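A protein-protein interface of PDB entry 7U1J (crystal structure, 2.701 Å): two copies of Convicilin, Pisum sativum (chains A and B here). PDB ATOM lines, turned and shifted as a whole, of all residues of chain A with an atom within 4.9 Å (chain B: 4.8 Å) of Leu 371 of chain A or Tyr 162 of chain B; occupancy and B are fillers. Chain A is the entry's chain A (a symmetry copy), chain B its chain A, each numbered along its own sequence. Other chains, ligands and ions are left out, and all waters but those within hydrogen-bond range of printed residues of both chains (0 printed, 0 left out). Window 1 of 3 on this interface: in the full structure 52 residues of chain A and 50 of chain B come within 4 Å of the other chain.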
ATOM      1  N   PRO A 284     -25.309 -26.226  18.434  1.00  0.00           N
ATOM      2  CA  PRO A 284     -26.250 -25.133  18.206  1.00  0.00           C
ATOM      3  C   PRO A 284     -27.344 -25.576  17.231  1.00  0.00           C
ATOM      4  O   PRO A 284     -27.041 -26.235  16.250  1.00  0.00           O
ATOM      5  CB  PRO A 284     -25.425 -23.978  17.606  1.00  0.00           C
ATOM      6  CG  PRO A 284     -23.983 -24.328  17.906  1.00  0.00           C
ATOM      7  CD  PRO A 284     -23.914 -25.807  18.253  1.00  0.00           C
ATOM      8  N   HIS A 285     -28.584 -25.198  17.528  1.00  0.00           N
ATOM      9  CA  HIS A 285     -29.752 -25.374  16.622  1.00  0.00           C
ATOM     10  C   HIS A 285     -30.924 -24.495  17.026  1.00  0.00           C
ATOM     11  O   HIS A 285     -30.967 -24.034  18.163  1.00  0.00           O
ATOM     12  CB  HIS A 285     -30.239 -26.808  16.687  1.00  0.00           C
ATOM     13  CG  HIS A 285     -30.703 -27.187  18.036  1.00  0.00           C
ATOM     14  ND1 HIS A 285     -29.845 -27.351  19.063  1.00  0.00           N
ATOM     15  CD2 HIS A 285     -31.933 -27.427  18.522  1.00  0.00           C
ATOM     16  CE1 HIS A 285     -30.530 -27.728  20.128  1.00  0.00           C
ATOM     17  NE2 HIS A 285     -31.810 -27.772  19.825  1.00  0.00           N
ATOM     18  N   TYR A 286     -31.897 -24.360  16.139  1.00  0.00           N
ATOM     19  CA  TYR A 286     -33.219 -23.769  16.483  1.00  0.00           C
ATOM     20  C   TYR A 286     -34.297 -24.772  16.061  1.00  0.00           C
ATOM     21  O   TYR A 286     -34.044 -25.550  15.116  1.00  0.00           O
ATOM     22  CB  TYR A 286     -33.362 -22.381  15.852  1.00  0.00           C
ATOM     23  CG  TYR A 286     -33.471 -22.353  14.345  1.00  0.00           C
ATOM     24  CD1 TYR A 286     -34.651 -22.735  13.737  1.00  0.00           C
ATOM     25  CD2 TYR A 286     -32.451 -21.878  13.521  1.00  0.00           C
ATOM     26  CE1 TYR A 286     -34.806 -22.683  12.367  1.00  0.00           C
ATOM     27  CE2 TYR A 286     -32.588 -21.820  12.142  1.00  0.00           C
ATOM     28  CZ  TYR A 286     -33.778 -22.225  11.563  1.00  0.00           C
ATOM     29  OH  TYR A 286     -34.034 -22.197  10.222  1.00  0.00           O
ATOM     30  N   LEU A 306     -30.026 -17.696  22.309  1.00  0.00           N
ATOM     31  CA  LEU A 306     -29.931 -16.443  21.538  1.00  0.00           C
ATOM     32  C   LEU A 306     -31.344 -15.990  21.236  1.00  0.00           C
ATOM     33  O   LEU A 306     -32.092 -16.766  20.654  1.00  0.00           O
ATOM     34  CB  LEU A 306     -29.183 -16.702  20.227  1.00  0.00           C
ATOM     35  CG  LEU A 306     -27.766 -17.271  20.354  1.00  0.00           C
ATOM     36  CD1 LEU A 306     -27.065 -17.151  18.995  1.00  0.00           C
ATOM     37  CD2 LEU A 306     -26.967 -16.566  21.450  1.00  0.00           C
ATOM     38  N   VAL A 325     -28.998  -8.866  18.781  1.00  0.00           N
ATOM     39  CA  VAL A 325     -29.055 -10.272  19.273  1.00  0.00           C
ATOM     40  C   VAL A 325     -28.514 -10.279  20.702  1.00  0.00           C
ATOM     41  O   VAL A 325     -27.496  -9.645  20.940  1.00  0.00           O
ATOM     42  CB  VAL A 325     -28.292 -11.227  18.331  1.00  0.00           C
ATOM     43  CG1 VAL A 325     -28.254 -12.646  18.862  1.00  0.00           C
ATOM     44  CG2 VAL A 325     -28.887 -11.235  16.926  1.00  0.00           C
ATOM     45  N   PRO A 345     -31.962 -19.794  18.387  1.00  0.00           N
ATOM     46  CA  PRO A 345     -30.794 -20.686  18.420  1.00  0.00           C
ATOM     47  C   PRO A 345     -30.428 -21.006  19.860  1.00  0.00           C
ATOM     48  O   PRO A 345     -30.567 -20.123  20.678  1.00  0.00           O
ATOM     49  CB  PRO A 345     -29.698 -19.843  17.777  1.00  0.00           C
ATOM     50  CG  PRO A 345     -30.473 -18.933  16.843  1.00  0.00           C
ATOM     51  CD  PRO A 345     -31.707 -18.560  17.634  1.00  0.00           C
ATOM     52  N   ASN A 369     -33.052 -27.377  13.062  1.00  0.00           N
ATOM     53  CA  ASN A 369     -32.009 -26.839  12.171  1.00  0.00           C
ATOM     54  C   ASN A 369     -30.722 -26.687  12.986  1.00  0.00           C
ATOM     55  O   ASN A 369     -30.648 -25.788  13.805  1.00  0.00           O
ATOM     56  CB  ASN A 369     -32.434 -25.493  11.596  1.00  0.00           C
ATOM     57  CG  ASN A 369     -33.503 -25.593  10.532  1.00  0.00           C
ATOM     58  OD1 ASN A 369     -33.224 -25.304   9.366  1.00  0.00           O
ATOM     59  ND2 ASN A 369     -34.718 -25.973  10.908  1.00  0.00           N
ATOM     60  N   PHE A 370     -29.750 -27.577  12.818  1.00  0.00           N
ATOM     61  CA  PHE A 370     -28.406 -27.416  13.414  1.00  0.00           C
ATOM     62  C   PHE A 370     -27.608 -26.432  12.561  1.00  0.00           C
ATOM     63  O   PHE A 370     -27.911 -26.227  11.351  1.00  0.00           O
ATOM     64  CB  PHE A 370     -27.764 -28.783  13.598  1.00  0.00           C
ATOM     65  CG  PHE A 370     -28.416 -29.561  14.713  1.00  0.00           C
ATOM     66  CD1 PHE A 370     -29.634 -30.198  14.520  1.00  0.00           C
ATOM     67  CD2 PHE A 370     -27.841 -29.611  15.974  1.00  0.00           C
ATOM     68  CE1 PHE A 370     -30.239 -30.896  15.555  1.00  0.00           C
ATOM     69  CE2 PHE A 370     -28.473 -30.281  17.014  1.00  0.00           C
ATOM     70  CZ  PHE A 370     -29.673 -30.911  16.806  1.00  0.00           C
ATOM     71  N   LEU A 371     -26.651 -25.780  13.216  1.00  0.00           N
ATOM     72  CA  LEU A 371     -25.768 -24.762  12.613  1.00  0.00           C
ATOM     73  C   LEU A 371     -24.319 -25.252  12.625  1.00  0.00           C
ATOM     74  O   LEU A 371     -23.443 -24.454  12.246  1.00  0.00           O
ATOM     75  CB  LEU A 371     -25.947 -23.468  13.398  1.00  0.00           C
ATOM     76  CG  LEU A 371     -27.389 -22.960  13.408  1.00  0.00           C
ATOM     77  CD1 LEU A 371     -27.589 -21.926  14.499  1.00  0.00           C
ATOM     78  CD2 LEU A 371     -27.739 -22.376  12.070  1.00  0.00           C
ATOM     79  N   SER A 372     -24.102 -26.529  12.944  1.00  0.00           N
ATOM     80  CA  SER A 372     -22.772 -27.173  12.900  1.00  0.00           C
ATOM     81  C   SER A 372     -22.927 -28.704  12.898  1.00  0.00           C
ATOM     82  O   SER A 372     -23.995 -29.201  13.340  1.00  0.00           O
ATOM     83  CB  SER A 372     -21.964 -26.708  14.054  1.00  0.00           C
ATOM     84  OG  SER A 372     -22.267 -27.509  15.164  1.00  0.00           O
ATOM     85  N   GLY A 373     -21.930 -29.448  12.404  1.00  0.00           N
ATOM     86  CA  GLY A 373     -22.004 -30.926  12.396  1.00  0.00           C
ATOM     87  C   GLY A 373     -22.503 -31.376  11.052  1.00  0.00           C
ATOM     88  O   GLY A 373     -22.763 -30.467  10.257  1.00  0.00           O
ATOM     89  N   ASN A 377     -27.941 -29.900   9.382  1.00  0.00           N
ATOM     90  CA  ASN A 377     -27.131 -28.665   9.350  1.00  0.00           C
ATOM     91  C   ASN A 377     -27.650 -27.788   8.203  1.00  0.00           C
ATOM     92  O   ASN A 377     -27.305 -27.993   7.013  1.00  0.00           O
ATOM     93  CB  ASN A 377     -25.641 -28.971   9.247  1.00  0.00           C
ATOM     94  CG  ASN A 377     -24.830 -27.695   9.283  1.00  0.00           C
ATOM     95  OD1 ASN A 377     -25.206 -26.691   8.671  1.00  0.00           O
ATOM     96  ND2 ASN A 377     -23.708 -27.719   9.981  1.00  0.00           N
ATOM     97  N   VAL A 378     -28.446 -26.794   8.548  1.00  0.00           N
ATOM     98  CA  VAL A 378     -29.096 -25.964   7.512  1.00  0.00           C
ATOM     99  C   VAL A 378     -28.035 -25.182   6.740  1.00  0.00           C
ATOM    100  O   VAL A 378     -28.328 -24.852   5.605  1.00  0.00           O
ATOM    101  CB  VAL A 378     -30.128 -25.046   8.155  1.00  0.00           C
ATOM    102  CG1 VAL A 378     -29.441 -24.056   9.060  1.00  0.00           C
ATOM    103  CG2 VAL A 378     -30.965 -24.373   7.103  1.00  0.00           C
ATOM    104  N   ILE A 379     -26.874 -24.866   7.324  1.00  0.00           N
ATOM    105  CA  ILE A 379     -25.812 -24.082   6.619  1.00  0.00           C
ATOM    106  C   ILE A 379     -25.310 -24.862   5.383  1.00  0.00           C
ATOM    107  O   ILE A 379     -25.283 -24.261   4.275  1.00  0.00           O
ATOM    108  CB  ILE A 379     -24.668 -23.713   7.564  1.00  0.00           C
ATOM    109  CG1 ILE A 379     -25.118 -22.708   8.616  1.00  0.00           C
ATOM    110  CG2 ILE A 379     -23.505 -23.175   6.778  1.00  0.00           C
ATOM    111  CD1 ILE A 379     -24.006 -22.199   9.492  1.00  0.00           C
ATOM    112  N   HIS B  81     -34.034 -16.383   8.830  1.00  0.00           N
ATOM    113  CA  HIS B  81     -35.284 -17.104   9.166  1.00  0.00           C
ATOM    114  C   HIS B  81     -36.130 -16.168  10.006  1.00  0.00           C
ATOM    115  O   HIS B  81     -35.546 -15.359  10.765  1.00  0.00           O
ATOM    116  CB  HIS B  81     -35.024 -18.474   9.786  1.00  0.00           C
ATOM    117  CG  HIS B  81     -34.580 -18.474  11.202  1.00  0.00           C
ATOM    118  ND1 HIS B  81     -33.259 -18.637  11.555  1.00  0.00           N
ATOM    119  CD2 HIS B  81     -35.287 -18.414  12.355  1.00  0.00           C
ATOM    120  CE1 HIS B  81     -33.169 -18.659  12.867  1.00  0.00           C
ATOM    121  NE2 HIS B  81     -34.403 -18.505  13.383  1.00  0.00           N
ATOM    122  N   PHE B 153     -34.026 -13.557  12.300  1.00  0.00           N
ATOM    123  CA  PHE B 153     -32.725 -14.084  12.750  1.00  0.00           C
ATOM    124  C   PHE B 153     -31.837 -14.148  11.523  1.00  0.00           C
ATOM    125  O   PHE B 153     -32.152 -14.905  10.602  1.00  0.00           O
ATOM    126  CB  PHE B 153     -32.918 -15.451  13.416  1.00  0.00           C
ATOM    127  CG  PHE B 153     -33.375 -15.350  14.845  1.00  0.00           C
ATOM    128  CD1 PHE B 153     -32.499 -14.930  15.829  1.00  0.00           C
ATOM    129  CD2 PHE B 153     -34.686 -15.600  15.190  1.00  0.00           C
ATOM    130  CE1 PHE B 153     -32.906 -14.812  17.145  1.00  0.00           C
ATOM    131  CE2 PHE B 153     -35.098 -15.484  16.506  1.00  0.00           C
ATOM    132  CZ  PHE B 153     -34.214 -15.075  17.477  1.00  0.00           C
ATOM    133  N   ASP B 154     -30.771 -13.361  11.517  1.00  0.00           N
ATOM    134  CA  ASP B 154     -29.906 -13.163  10.330  1.00  0.00           C
ATOM    135  C   ASP B 154     -28.738 -14.148  10.395  1.00  0.00           C
ATOM    136  O   ASP B 154     -27.956 -14.016  11.330  1.00  0.00           O
ATOM    137  CB  ASP B 154     -29.450 -11.713  10.259  1.00  0.00           C
ATOM    138  CG  ASP B 154     -29.694 -11.173   8.880  1.00  0.00           C
ATOM    139  OD1 ASP B 154     -29.113 -11.781   7.903  1.00  0.00           O
ATOM    140  OD2 ASP B 154     -30.539 -10.227   8.781  1.00  0.00           O
ATOM    141  N   LEU B 155     -28.673 -15.131   9.482  1.00  0.00           N
ATOM    142  CA  LEU B 155     -27.568 -16.125   9.412  1.00  0.00           C
ATOM    143  C   LEU B 155     -26.329 -15.459   8.803  1.00  0.00           C
ATOM    144  O   LEU B 155     -25.258 -15.619   9.326  1.00  0.00           O
ATOM    145  CB  LEU B 155     -28.038 -17.295   8.560  1.00  0.00           C
ATOM    146  CG  LEU B 155     -27.087 -18.485   8.474  1.00  0.00           C
ATOM    147  CD1 LEU B 155     -26.613 -18.863   9.849  1.00  0.00           C
ATOM    148  CD2 LEU B 155     -27.759 -19.657   7.803  1.00  0.00           C
ATOM    149  N   ASN B 160     -26.119  -7.868  13.080  1.00  0.00           N
ATOM    150  CA  ASN B 160     -27.026  -8.747  13.858  1.00  0.00           C
ATOM    151  C   ASN B 160     -26.923 -10.220  13.438  1.00  0.00           C
ATOM    152  O   ASN B 160     -27.876 -10.993  13.685  1.00  0.00           O
ATOM    153  CB  ASN B 160     -28.470  -8.285  13.702  1.00  0.00           C
ATOM    154  CG  ASN B 160     -28.665  -6.832  14.071  1.00  0.00           C
ATOM    155  OD1 ASN B 160     -29.501  -6.153  13.463  1.00  0.00           O
ATOM    156  ND2 ASN B 160     -27.916  -6.369  15.065  1.00  0.00           N
ATOM    157  N   GLN B 161     -25.799 -10.633  12.877  1.00  0.00           N
ATOM    158  CA  GLN B 161     -25.602 -12.063  12.602  1.00  0.00           C
ATOM    159  C   GLN B 161     -25.696 -12.790  13.927  1.00  0.00           C
ATOM    160  O   GLN B 161     -24.858 -12.523  14.772  1.00  0.00           O
ATOM    161  CB  GLN B 161     -24.254 -12.329  11.962  1.00  0.00           C
ATOM    162  CG  GLN B 161     -24.037 -13.801  11.656  1.00  0.00           C
ATOM    163  CD  GLN B 161     -22.710 -13.985  10.972  1.00  0.00           C
ATOM    164  OE1 GLN B 161     -21.718 -13.396  11.373  1.00  0.00           O
ATOM    165  NE2 GLN B 161     -22.696 -14.780   9.919  1.00  0.00           N
ATOM    166  N   TYR B 162     -26.645 -13.708  14.053  1.00  0.00           N
ATOM    167  CA  TYR B 162     -26.998 -14.383  15.319  1.00  0.00           C
ATOM    168  C   TYR B 162     -25.893 -15.346  15.779  1.00  0.00           C
ATOM    169  O   TYR B 162     -25.697 -15.465  16.989  1.00  0.00           O
ATOM    170  CB  TYR B 162     -28.402 -14.968  15.198  1.00  0.00           C
ATOM    171  CG  TYR B 162     -28.593 -16.166  14.311  1.00  0.00           C
ATOM    172  CD1 TYR B 162     -28.126 -17.423  14.654  1.00  0.00           C
ATOM    173  CD2 TYR B 162     -29.335 -16.053  13.145  1.00  0.00           C
ATOM    174  CE1 TYR B 162     -28.371 -18.522  13.854  1.00  0.00           C
ATOM    175  CE2 TYR B 162     -29.580 -17.146  12.324  1.00  0.00           C
ATOM    176  CZ  TYR B 162     -29.091 -18.390  12.676  1.00  0.00           C
ATOM    177  OH  TYR B 162     -29.377 -19.461  11.871  1.00  0.00           O
ATOM    178  N   LEU B 163     -25.114 -15.941  14.886  1.00  0.00           N
ATOM    179  CA  LEU B 163     -24.007 -16.866  15.269  1.00  0.00           C
ATOM    180  C   LEU B 163     -23.019 -16.151  16.187  1.00  0.00           C
ATOM    181  O   LEU B 163     -22.322 -16.869  16.944  1.00  0.00           O
ATOM    182  CB  LEU B 163     -23.287 -17.388  14.018  1.00  0.00           C
ATOM    183  CG  LEU B 163     -24.083 -18.382  13.174  1.00  0.00           C
ATOM    184  CD1 LEU B 163     -23.286 -18.805  11.958  1.00  0.00           C
ATOM    185  CD2 LEU B 163     -24.462 -19.595  14.002  1.00  0.00           C
ATOM    186  N   ARG B 164     -22.950 -14.816  16.143  1.00  0.00           N
ATOM    187  CA  ARG B 164     -21.956 -14.052  16.966  1.00  0.00           C
ATOM    188  C   ARG B 164     -22.393 -14.025  18.436  1.00  0.00           C
ATOM    189  O   ARG B 164     -21.551 -13.758  19.298  1.00  0.00           O
ATOM    190  CB  ARG B 164     -21.744 -12.622  16.479  1.00  0.00           C
ATOM    191  CG  ARG B 164     -21.403 -12.534  15.004  1.00  0.00           C
ATOM    192  CD  ARG B 164     -21.171 -11.090  14.645  1.00  0.00           C
ATOM    193  NE  ARG B 164     -20.953 -10.959  13.211  1.00  0.00           N
ATOM    194  CZ  ARG B 164     -20.901  -9.806  12.546  1.00  0.00           C
ATOM    195  NH1 ARG B 164     -21.032  -8.652  13.182  1.00  0.00           N
ATOM    196  NH2 ARG B 164     -20.706  -9.820  11.237  1.00  0.00           N
ATOM    197  N   GLY B 165     -23.658 -14.345  18.701  1.00  0.00           N
ATOM    198  CA  GLY B 165     -24.233 -14.340  20.057  1.00  0.00           C
ATOM    199  C   GLY B 165     -23.660 -15.436  20.926  1.00  0.00           C
ATOM    200  O   GLY B 165     -23.794 -15.352  22.116  1.00  0.00           O
ATOM    201  N   PHE B 166     -23.103 -16.481  20.333  1.00  0.00           N
ATOM    202  CA  PHE B 166     -22.539 -17.626  21.084  1.00  0.00           C
ATOM    203  C   PHE B 166     -21.130 -17.254  21.572  1.00  0.00           C
ATOM    204  O   PHE B 166     -20.289 -16.634  20.824  1.00  0.00           O
ATOM    205  CB  PHE B 166     -22.518 -18.862  20.181  1.00  0.00           C
ATOM    206  CG  PHE B 166     -23.863 -19.479  19.907  1.00  0.00           C
ATOM    207  CD1 PHE B 166     -24.678 -19.892  20.953  1.00  0.00           C
ATOM    208  CD2 PHE B 166     -24.271 -19.725  18.610  1.00  0.00           C
ATOM    209  CE1 PHE B 166     -25.897 -20.499  20.702  1.00  0.00           C
ATOM    210  CE2 PHE B 166     -25.476 -20.350  18.366  1.00  0.00           C
ATOM    211  CZ  PHE B 166     -26.282 -20.715  19.406  1.00  0.00           C
ATOM    212  N   TYR B 175     -18.066 -25.797  16.082  1.00  0.00           N
ATOM    213  CA  TYR B 175     -17.490 -25.961  14.710  1.00  0.00           C
ATOM    214  C   TYR B 175     -16.197 -26.794  14.693  1.00  0.00           C
ATOM    215  O   TYR B 175     -15.783 -27.219  13.594  1.00  0.00           O
ATOM    216  CB  TYR B 175     -17.293 -24.591  14.081  1.00  0.00           C
ATOM    217  CG  TYR B 175     -18.622 -23.952  13.819  1.00  0.00           C
ATOM    218  CD1 TYR B 175     -19.361 -24.348  12.728  1.00  0.00           C
ATOM    219  CD2 TYR B 175     -19.170 -23.037  14.707  1.00  0.00           C
ATOM    220  CE1 TYR B 175     -20.597 -23.790  12.481  1.00  0.00           C
ATOM    221  CE2 TYR B 175     -20.408 -22.475  14.474  1.00  0.00           C
ATOM    222  CZ  TYR B 175     -21.127 -22.865  13.363  1.00  0.00           C
ATOM    223  OH  TYR B 175     -22.355 -22.338  13.099  1.00  0.00           O
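The backbone carbonyl oxygen (O) of Leu 371 of chain A sits at hydrogen-bond distance from the side-chain hydroxyl (OH) of Tyr 175 of chain B (2.5 Å).
The backbone carbonyl oxygen of His 81 of chain B is in hydrogen-bond range of the backbone NH of Phe 153 of chain B (2.8 Å).
The backbone carbonyl oxygen (O) of Asp 154 of chain B lies within hydrogen-bond range of the backbone NH (N) of Tyr 162 of chain B, at 3.0 Å.
O of Pro 284 of chain A is in hydrogen-bond range of N of Leu 371 of chain A (3.1 Å).
O of Tyr 286 of chain A is in hydrogen-bond range of N of Asn 369 of chain A, at 2.9 Å.
N of Ser 372 of chain A sits close to ND2 of Asn 377 of chain A (3.2 Å).
The side-chain amide oxygen (OD1) of Asn 377 of chain A sits at hydrogen-bond distance from the backbone NH (N) of Ile 379 of chain A, at 2.8 Å.
Phe 166 of chain B touches Pro 284 of chain A (CE2 to CB, 3.7 Å).
CE2 of Tyr 286 of chain A touches CE1 of His 81 of chain B, at 3.3 Å.
Tyr 162 of chain B touches Leu 306 of chain A.
O of Gly 165 of chain B touches CD2 of Leu 306 of chain A, 3.5 Å away.
Leu 306 of chain A touches Phe 166 of chain B (CD1 to CE2, 3.6 Å).
Val 325 of chain A touches Asn 160 of chain B (CG2 to O, 3.4 Å).
Phe 153 of chain B touches Pro 345 of chain A (CE1 to CD, 3.97 Å).
Leu 371 of chain A touches Tyr 162 of chain B.
Leu 163 of chain B touches Leu 371 of chain A.
CD1 of Ile 379 of chain A touches OH of Tyr 175 of chain B (3.97 Å).
Printed residues of chain B within 4 Å of Val 325 of chain A: Asn 160 (3.4 Å).
Of the printed residues of chain A, Tyr 162 of chain B touches Tyr 286 (3.99 Å), Leu 306 (3.0 Å), Pro 345 (3.5 Å) and Leu 371 (3.3 Å).
Of the printed residues of chain A, Gly 165 of chain B touches Leu 306.
The nearest residue of chain B that does not touch Leu 371 of chain A is Leu 155 of chain B (4.3 Å).
Hydrophobic or aromatic side chains of chain A that line the printed part of chain B: Pro 284, Tyr 286, Leu 306, Val 325, Pro 345, Leu 371 and Ile 379.
Along chain A the printed residues that touch a printed residue of chain B span positions 284 to 379.
Of the 12 printed residues of chain B, 8 touch a printed residue of chain A.
Printed residues of chain B that touch a printed residue of chain A: His 81, Phe 153, Asn 160, Tyr 162, Leu 163, Gly 165, Phe 166 and Tyr 175.
Hydrophobic or aromatic side chains of chain B within 4 Å of the printed part of chain A: His 81, Phe 153, Tyr 162, Leu 163, Phe 166 and Tyr 175.
Among the printed residues, 15 pairs touch across the chains.
Among the printed residues, no Asp or Glu carboxylate lies within 4 Å of a Lys or Arg side-chain nitrogen of the other chain.
No position is printed for both chains.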
